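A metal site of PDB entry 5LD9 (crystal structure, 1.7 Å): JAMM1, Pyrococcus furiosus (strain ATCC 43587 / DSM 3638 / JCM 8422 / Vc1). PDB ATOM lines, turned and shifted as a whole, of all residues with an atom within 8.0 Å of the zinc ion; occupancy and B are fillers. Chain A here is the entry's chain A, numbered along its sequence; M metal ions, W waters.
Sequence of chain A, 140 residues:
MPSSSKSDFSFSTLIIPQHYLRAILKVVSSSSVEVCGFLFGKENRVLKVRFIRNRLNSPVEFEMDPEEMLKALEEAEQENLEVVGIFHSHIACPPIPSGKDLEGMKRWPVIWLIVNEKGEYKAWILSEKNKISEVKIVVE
The side-chain hydroxyl (OG) of Ser 98 lies within hydrogen-bond range of the backbone NH (N) of Asp 101, 3.0 Å away. A ring nitrogen (ND1) of His 90 sits at hydrogen-bond distance from the backbone carbonyl oxygen of Pro 94, at 2.9 Å. The backbone carbonyl oxygen (O) of Val 115 is in hydrogen-bond range of the backbone NH (N) of His 90, at 2.8 Å. O of His 88 lies within hydrogen-bond range of N of Val 115 (3.1 Å). N of His 88 lies within hydrogen-bond range of O of Leu 113, 3.0 Å away. OG of Ser 98 sits close to N of Lys 100 (3.4 Å).
The zinc ion is bound by OD2 of Asp 101 (2.0 Å), NE2 of His 90 (2.0 Å), NE2 of His 88 (2.1 Å) and water W1 (2.1 Å). Slightly farther from the zinc ion lies the side-chain carboxylate (OD1) of Asp 101 (2.7 Å).
Water W1 lies within hydrogen-bond range of OE1 of Glu 34 (2.9 Å) and OD1 of Asp 101 (3.3 Å).
OG of Ser 98 touches the zinc ion, at 3.9 Å. Within 4 Å of the zinc ion: His 88, His 90, Ser 98 and Asp 101. Along chain A the residues within 4 Å of the zinc ion span positions 88 to 101.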
ATOM      1  N   GLU A  34     -15.723   0.799  14.027  1.00  0.00           N
ATOM      2  CA  GLU A  34     -16.280   2.142  13.990  1.00  0.00           C
ATOM      3  C   GLU A  34     -15.330   3.065  13.238  1.00  0.00           C
ATOM      4  O   GLU A  34     -14.105   3.023  13.438  1.00  0.00           O
ATOM      5  CB  GLU A  34     -16.536   2.675  15.394  1.00  0.00           C
ATOM      6  CG  GLU A  34     -17.629   1.923  16.156  1.00  0.00           C
ATOM      7  CD  GLU A  34     -18.201   2.700  17.340  1.00  0.00           C
ATOM      8  OE1 GLU A  34     -17.664   3.786  17.679  1.00  0.00           O
ATOM      9  OE2 GLU A  34     -19.212   2.247  17.911  1.00  0.00           O
ATOM     10  N   VAL A  35     -15.905   3.902  12.377  1.00  0.00           N
ATOM     11  CA  VAL A  35     -15.206   4.925  11.607  1.00  0.00           C
ATOM     12  C   VAL A  35     -15.368   6.238  12.358  1.00  0.00           C
ATOM     13  O   VAL A  35     -16.346   6.430  13.079  1.00  0.00           O
ATOM     14  CB  VAL A  35     -15.768   5.003  10.173  1.00  0.00           C
ATOM     15  CG1 VAL A  35     -15.118   6.107   9.367  1.00  0.00           C
ATOM     16  CG2 VAL A  35     -15.613   3.648   9.481  1.00  0.00           C
ATOM     17  N   VAL A  60     -17.242  -1.434  18.475  1.00  0.00           N
ATOM     18  CA  VAL A  60     -18.202  -0.968  19.475  1.00  0.00           C
ATOM     19  C   VAL A  60     -17.780   0.320  20.157  1.00  0.00           C
ATOM     20  O   VAL A  60     -18.477   0.769  21.070  1.00  0.00           O
ATOM     21  CB  VAL A  60     -18.489  -2.065  20.516  1.00  0.00           C
ATOM     22  CG1 VAL A  60     -19.115  -3.270  19.853  1.00  0.00           C
ATOM     23  CG2 VAL A  60     -17.214  -2.445  21.252  1.00  0.00           C
ATOM     24  N   GLU A  61     -16.659   0.934  19.773  1.00  0.00           N
ATOM     25  CA  GLU A  61     -16.263   2.216  20.346  1.00  0.00           C
ATOM     26  C   GLU A  61     -15.153   2.800  19.473  1.00  0.00           C
ATOM     27  O   GLU A  61     -14.585   2.115  18.613  1.00  0.00           O
ATOM     28  CB  GLU A  61     -15.818   2.083  21.802  1.00  0.00           C
ATOM     29  CG  GLU A  61     -14.654   1.128  22.029  1.00  0.00           C
ATOM     30  CD  GLU A  61     -14.161   1.151  23.462  1.00  0.00           C
ATOM     31  OE1 GLU A  61     -14.803   1.801  24.315  1.00  0.00           O
ATOM     32  OE2 GLU A  61     -13.126   0.510  23.751  1.00  0.00           O
ATOM     33  N   PHE A  62     -14.862   4.076  19.684  1.00  0.00           N
ATOM     34  CA  PHE A  62     -13.829   4.736  18.908  1.00  0.00           C
ATOM     35  C   PHE A  62     -13.053   5.741  19.750  1.00  0.00           C
ATOM     36  O   PHE A  62     -13.559   6.299  20.722  1.00  0.00           O
ATOM     37  CB  PHE A  62     -14.400   5.465  17.672  1.00  0.00           C
ATOM     38  CG  PHE A  62     -14.936   6.849  17.947  1.00  0.00           C
ATOM     39  CD1 PHE A  62     -16.254   7.025  18.362  1.00  0.00           C
ATOM     40  CD2 PHE A  62     -14.141   7.967  17.762  1.00  0.00           C
ATOM     41  CE1 PHE A  62     -16.750   8.301  18.606  1.00  0.00           C
ATOM     42  CE2 PHE A  62     -14.637   9.243  18.007  1.00  0.00           C
ATOM     43  CZ  PHE A  62     -15.937   9.409  18.429  1.00  0.00           C
ATOM     44  N   HIS A  88     -18.883   9.813  13.456  1.00  0.00           N
ATOM     45  CA  HIS A  88     -18.448   8.443  13.661  1.00  0.00           C
ATOM     46  C   HIS A  88     -19.624   7.516  13.389  1.00  0.00           C
ATOM     47  O   HIS A  88     -20.754   7.966  13.167  1.00  0.00           O
ATOM     48  CB  HIS A  88     -17.871   8.216  15.072  1.00  0.00           C
ATOM     49  CG  HIS A  88     -18.898   8.106  16.164  1.00  0.00           C
ATOM     50  ND1 HIS A  88     -19.497   9.214  16.726  1.00  0.00           N
ATOM     51  CD2 HIS A  88     -19.367   7.041  16.842  1.00  0.00           C
ATOM     52  CE1 HIS A  88     -20.327   8.821  17.677  1.00  0.00           C
ATOM     53  NE2 HIS A  88     -20.272   7.511  17.761  1.00  0.00           N
ATOM     54  N   SER A  89     -19.331   6.228  13.367  1.00  0.00           N
ATOM     55  CA  SER A  89     -20.324   5.214  13.067  1.00  0.00           C
ATOM     56  C   SER A  89     -20.538   4.287  14.252  1.00  0.00           C
ATOM     57  O   SER A  89     -19.641   4.085  15.078  1.00  0.00           O
ATOM     58  CB  SER A  89     -19.916   4.394  11.848  1.00  0.00           C
ATOM     59  OG  SER A  89     -18.689   3.722  12.037  1.00  0.00           O
ATOM     60  N   HIS A  90     -21.749   3.734  14.310  1.00  0.00           N
ATOM     61  CA  HIS A  90     -22.063   2.555  15.084  1.00  0.00           C
ATOM     62  C   HIS A  90     -22.319   1.394  14.141  1.00  0.00           C
ATOM     63  O   HIS A  90     -22.740   1.595  12.999  1.00  0.00           O
ATOM     64  CB  HIS A  90     -23.317   2.768  15.941  1.00  0.00           C
ATOM     65  CG  HIS A  90     -23.131   3.794  17.009  1.00  0.00           C
ATOM     66  ND1 HIS A  90     -24.185   4.379  17.675  1.00  0.00           N
ATOM     67  CD2 HIS A  90     -22.006   4.355  17.524  1.00  0.00           C
ATOM     68  CE1 HIS A  90     -23.726   5.248  18.549  1.00  0.00           C
ATOM     69  NE2 HIS A  90     -22.404   5.247  18.481  1.00  0.00           N
ATOM     70  N   ILE A  91     -22.049   0.182  14.610  1.00  0.00           N
ATOM     71  CA  ILE A  91     -22.307  -1.026  13.832  1.00  0.00           C
ATOM     72  C   ILE A  91     -23.446  -1.772  14.514  1.00  0.00           C
ATOM     73  O   ILE A  91     -23.332  -2.193  15.665  1.00  0.00           O
ATOM     74  CB  ILE A  91     -21.058  -1.901  13.709  1.00  0.00           C
ATOM     75  CG1 ILE A  91     -19.924  -1.104  13.024  1.00  0.00           C
ATOM     76  CG2 ILE A  91     -21.367  -3.127  12.883  1.00  0.00           C
ATOM     77  CD1 ILE A  91     -18.611  -1.863  12.896  1.00  0.00           C
ATOM     78  N   PRO A  94     -28.422   1.832  16.829  1.00  0.00           N
ATOM     79  CA  PRO A  94     -28.965   3.106  16.308  1.00  0.00           C
ATOM     80  C   PRO A  94     -27.941   4.222  16.386  1.00  0.00           C
ATOM     81  O   PRO A  94     -27.025   4.190  17.217  1.00  0.00           O
ATOM     82  CB  PRO A  94     -30.163   3.391  17.233  1.00  0.00           C
ATOM     83  CG  PRO A  94     -30.515   2.073  17.827  1.00  0.00           C
ATOM     84  CD  PRO A  94     -29.234   1.311  17.946  1.00  0.00           C
ATOM     85  N   PRO A  95     -28.073   5.241  15.526  1.00  0.00           N
ATOM     86  CA  PRO A  95     -27.106   6.350  15.521  1.00  0.00           C
ATOM     87  C   PRO A  95     -27.415   7.375  16.611  1.00  0.00           C
ATOM     88  O   PRO A  95     -27.678   8.556  16.345  1.00  0.00           O
ATOM     89  CB  PRO A  95     -27.284   6.915  14.105  1.00  0.00           C
ATOM     90  CG  PRO A  95     -28.716   6.671  13.784  1.00  0.00           C
ATOM     91  CD  PRO A  95     -29.089   5.380  14.473  1.00  0.00           C
ATOM     92  N   ILE A  96     -27.360   6.913  17.861  1.00  0.00           N
ATOM     93  CA  ILE A  96     -27.750   7.694  19.034  1.00  0.00           C
ATOM     94  C   ILE A  96     -26.564   7.698  19.991  1.00  0.00           C
ATOM     95  O   ILE A  96     -25.864   6.682  20.107  1.00  0.00           O
ATOM     96  CB  ILE A  96     -29.011   7.108  19.684  1.00  0.00           C
ATOM     97  CG1 ILE A  96     -30.157   7.066  18.639  1.00  0.00           C
ATOM     98  CG2 ILE A  96     -29.449   7.920  20.872  1.00  0.00           C
ATOM     99  CD1 ILE A  96     -31.396   6.329  19.089  1.00  0.00           C
ATOM    100  N   PRO A  97     -26.276   8.789  20.709  1.00  0.00           N
ATOM    101  CA  PRO A  97     -25.038   8.827  21.509  1.00  0.00           C
ATOM    102  C   PRO A  97     -24.983   7.736  22.570  1.00  0.00           C
ATOM    103  O   PRO A  97     -25.933   7.554  23.345  1.00  0.00           O
ATOM    104  CB  PRO A  97     -25.076  10.219  22.140  1.00  0.00           C
ATOM    105  CG  PRO A  97     -25.903  11.032  21.219  1.00  0.00           C
ATOM    106  CD  PRO A  97     -26.971  10.082  20.730  1.00  0.00           C
ATOM    107  N   SER A  98     -23.853   7.041  22.616  1.00  0.00           N
ATOM    108  CA  SER A  98     -23.526   6.146  23.714  1.00  0.00           C
ATOM    109  C   SER A  98     -23.138   6.969  24.935  1.00  0.00           C
ATOM    110  O   SER A  98     -23.011   8.199  24.882  1.00  0.00           O
ATOM    111  CB  SER A  98     -22.370   5.225  23.324  1.00  0.00           C
ATOM    112  OG  SER A  98     -21.166   5.971  23.215  1.00  0.00           O
ATOM    113  N   GLY A  99     -22.921   6.276  26.055  1.00  0.00           N
ATOM    114  CA  GLY A  99     -22.435   6.964  27.239  1.00  0.00           C
ATOM    115  C   GLY A  99     -21.061   7.567  27.032  1.00  0.00           C
ATOM    116  O   GLY A  99     -20.778   8.683  27.474  1.00  0.00           O
ATOM    117  N   LYS A 100     -20.177   6.822  26.360  1.00  0.00           N
ATOM    118  CA  LYS A 100     -18.855   7.358  26.029  1.00  0.00           C
ATOM    119  C   LYS A 100     -18.975   8.549  25.096  1.00  0.00           C
ATOM    120  O   LYS A 100     -18.230   9.530  25.229  1.00  0.00           O
ATOM    121  CB  LYS A 100     -17.997   6.278  25.370  1.00  0.00           C
ATOM    122  CG  LYS A 100     -16.864   5.743  26.210  1.00  0.00           C
ATOM    123  CD  LYS A 100     -15.875   4.950  25.354  1.00  0.00           C
ATOM    124  CE  LYS A 100     -15.149   5.846  24.352  1.00  0.00           C
ATOM    125  NZ  LYS A 100     -14.154   5.121  23.518  1.00  0.00           N
ATOM    126  N   ASP A 101     -19.905   8.497  24.141  1.00  0.00           N
ATOM    127  CA  ASP A 101     -20.095   9.620  23.239  1.00  0.00           C
ATOM    128  C   ASP A 101     -20.465  10.880  24.016  1.00  0.00           C
ATOM    129  O   ASP A 101     -19.969  11.973  23.698  1.00  0.00           O
ATOM    130  CB  ASP A 101     -21.180   9.312  22.212  1.00  0.00           C
ATOM    131  CG  ASP A 101     -20.778   8.254  21.209  1.00  0.00           C
ATOM    132  OD1 ASP A 101     -19.577   8.004  20.987  1.00  0.00           O
ATOM    133  OD2 ASP A 101     -21.704   7.661  20.659  1.00  0.00           O
ATOM    134  N   LEU A 102     -21.331  10.742  25.021  1.00  0.00           N
ATOM    135  CA  LEU A 102     -21.732  11.911  25.807  1.00  0.00           C
ATOM    136  C   LEU A 102     -20.525  12.545  26.492  1.00  0.00           C
ATOM    137  O   LEU A 102     -20.403  13.772  26.530  1.00  0.00           O
ATOM    138  CB  LEU A 102     -22.777  11.522  26.854  1.00  0.00           C
ATOM    139  CG  LEU A 102     -23.201  12.644  27.819  1.00  0.00           C
ATOM    140  CD1 LEU A 102     -23.783  13.817  27.036  1.00  0.00           C
ATOM    141  CD2 LEU A 102     -24.189  12.136  28.856  1.00  0.00           C
ATOM    142  N   TRP A 112     -22.236  16.400  16.688  1.00  0.00           N
ATOM    143  CA  TRP A 112     -21.828  15.012  16.562  1.00  0.00           C
ATOM    144  C   TRP A 112     -22.766  14.313  15.572  1.00  0.00           C
ATOM    145  O   TRP A 112     -23.943  14.080  15.873  1.00  0.00           O
ATOM    146  CB  TRP A 112     -21.824  14.314  17.926  1.00  0.00           C
ATOM    147  CG  TRP A 112     -20.590  14.596  18.723  1.00  0.00           C
ATOM    148  CD1 TRP A 112     -20.088  15.829  19.062  1.00  0.00           C
ATOM    149  CD2 TRP A 112     -19.693  13.637  19.298  1.00  0.00           C
ATOM    150  NE1 TRP A 112     -18.938  15.684  19.795  1.00  0.00           N
ATOM    151  CE2 TRP A 112     -18.678  14.350  19.965  1.00  0.00           C
ATOM    152  CE3 TRP A 112     -19.665  12.243  19.321  1.00  0.00           C
ATOM    153  CZ2 TRP A 112     -17.629  13.714  20.633  1.00  0.00           C
ATOM    154  CZ3 TRP A 112     -18.626  11.609  19.988  1.00  0.00           C
ATOM    155  CH2 TRP A 112     -17.628  12.341  20.628  1.00  0.00           C
ATOM    156  N   LEU A 113     -22.235  13.996  14.407  1.00  0.00           N
ATOM    157  CA  LEU A 113     -22.951  13.212  13.399  1.00  0.00           C
ATOM    158  C   LEU A 113     -22.659  11.731  13.635  1.00  0.00           C
ATOM    159  O   LEU A 113     -21.498  11.320  13.670  1.00  0.00           O
ATOM    160  CB  LEU A 113     -22.532  13.613  11.999  1.00  0.00           C
ATOM    161  CG  LEU A 113     -23.010  12.735  10.838  1.00  0.00           C
ATOM    162  CD1 LEU A 113     -24.508  12.867  10.668  1.00  0.00           C
ATOM    163  CD2 LEU A 113     -22.280  13.095   9.571  1.00  0.00           C
ATOM    164  N   ILE A 114     -23.708  10.933  13.754  1.00  0.00           N
ATOM    165  CA  ILE A 114     -23.572   9.500  13.957  1.00  0.00           C
ATOM    166  C   ILE A 114     -24.304   8.788  12.828  1.00  0.00           C
ATOM    167  O   ILE A 114     -25.438   9.151  12.497  1.00  0.00           O
ATOM    168  CB  ILE A 114     -24.104   9.051  15.324  1.00  0.00           C
ATOM    169  CG1 ILE A 114     -23.549   9.970  16.423  1.00  0.00           C
ATOM    170  CG2 ILE A 114     -23.750   7.593  15.551  1.00  0.00           C
ATOM    171  CD1 ILE A 114     -23.980   9.560  17.857  1.00  0.00           C
ATOM    172  N   VAL A 115     -23.664   7.777  12.264  1.00  0.00           N
ATOM    173  CA  VAL A 115     -24.228   6.970  11.191  1.00  0.00           C
ATOM    174  C   VAL A 115     -24.052   5.501  11.549  1.00  0.00           C
ATOM    175  O   VAL A 115     -23.305   5.155  12.473  1.00  0.00           O
ATOM    176  CB  VAL A 115     -23.570   7.271   9.821  1.00  0.00           C
ATOM    177  CG1 VAL A 115     -23.546   8.766   9.549  1.00  0.00           C
ATOM    178  CG2 VAL A 115     -22.159   6.691   9.725  1.00  0.00           C
HETATM  179 ZN    ZN M   1     -20.920   6.369  19.340  1.00  0.00          ZN
HETATM  180  O   HOH W   1     -19.358   5.039  19.670  1.00  0.00           O
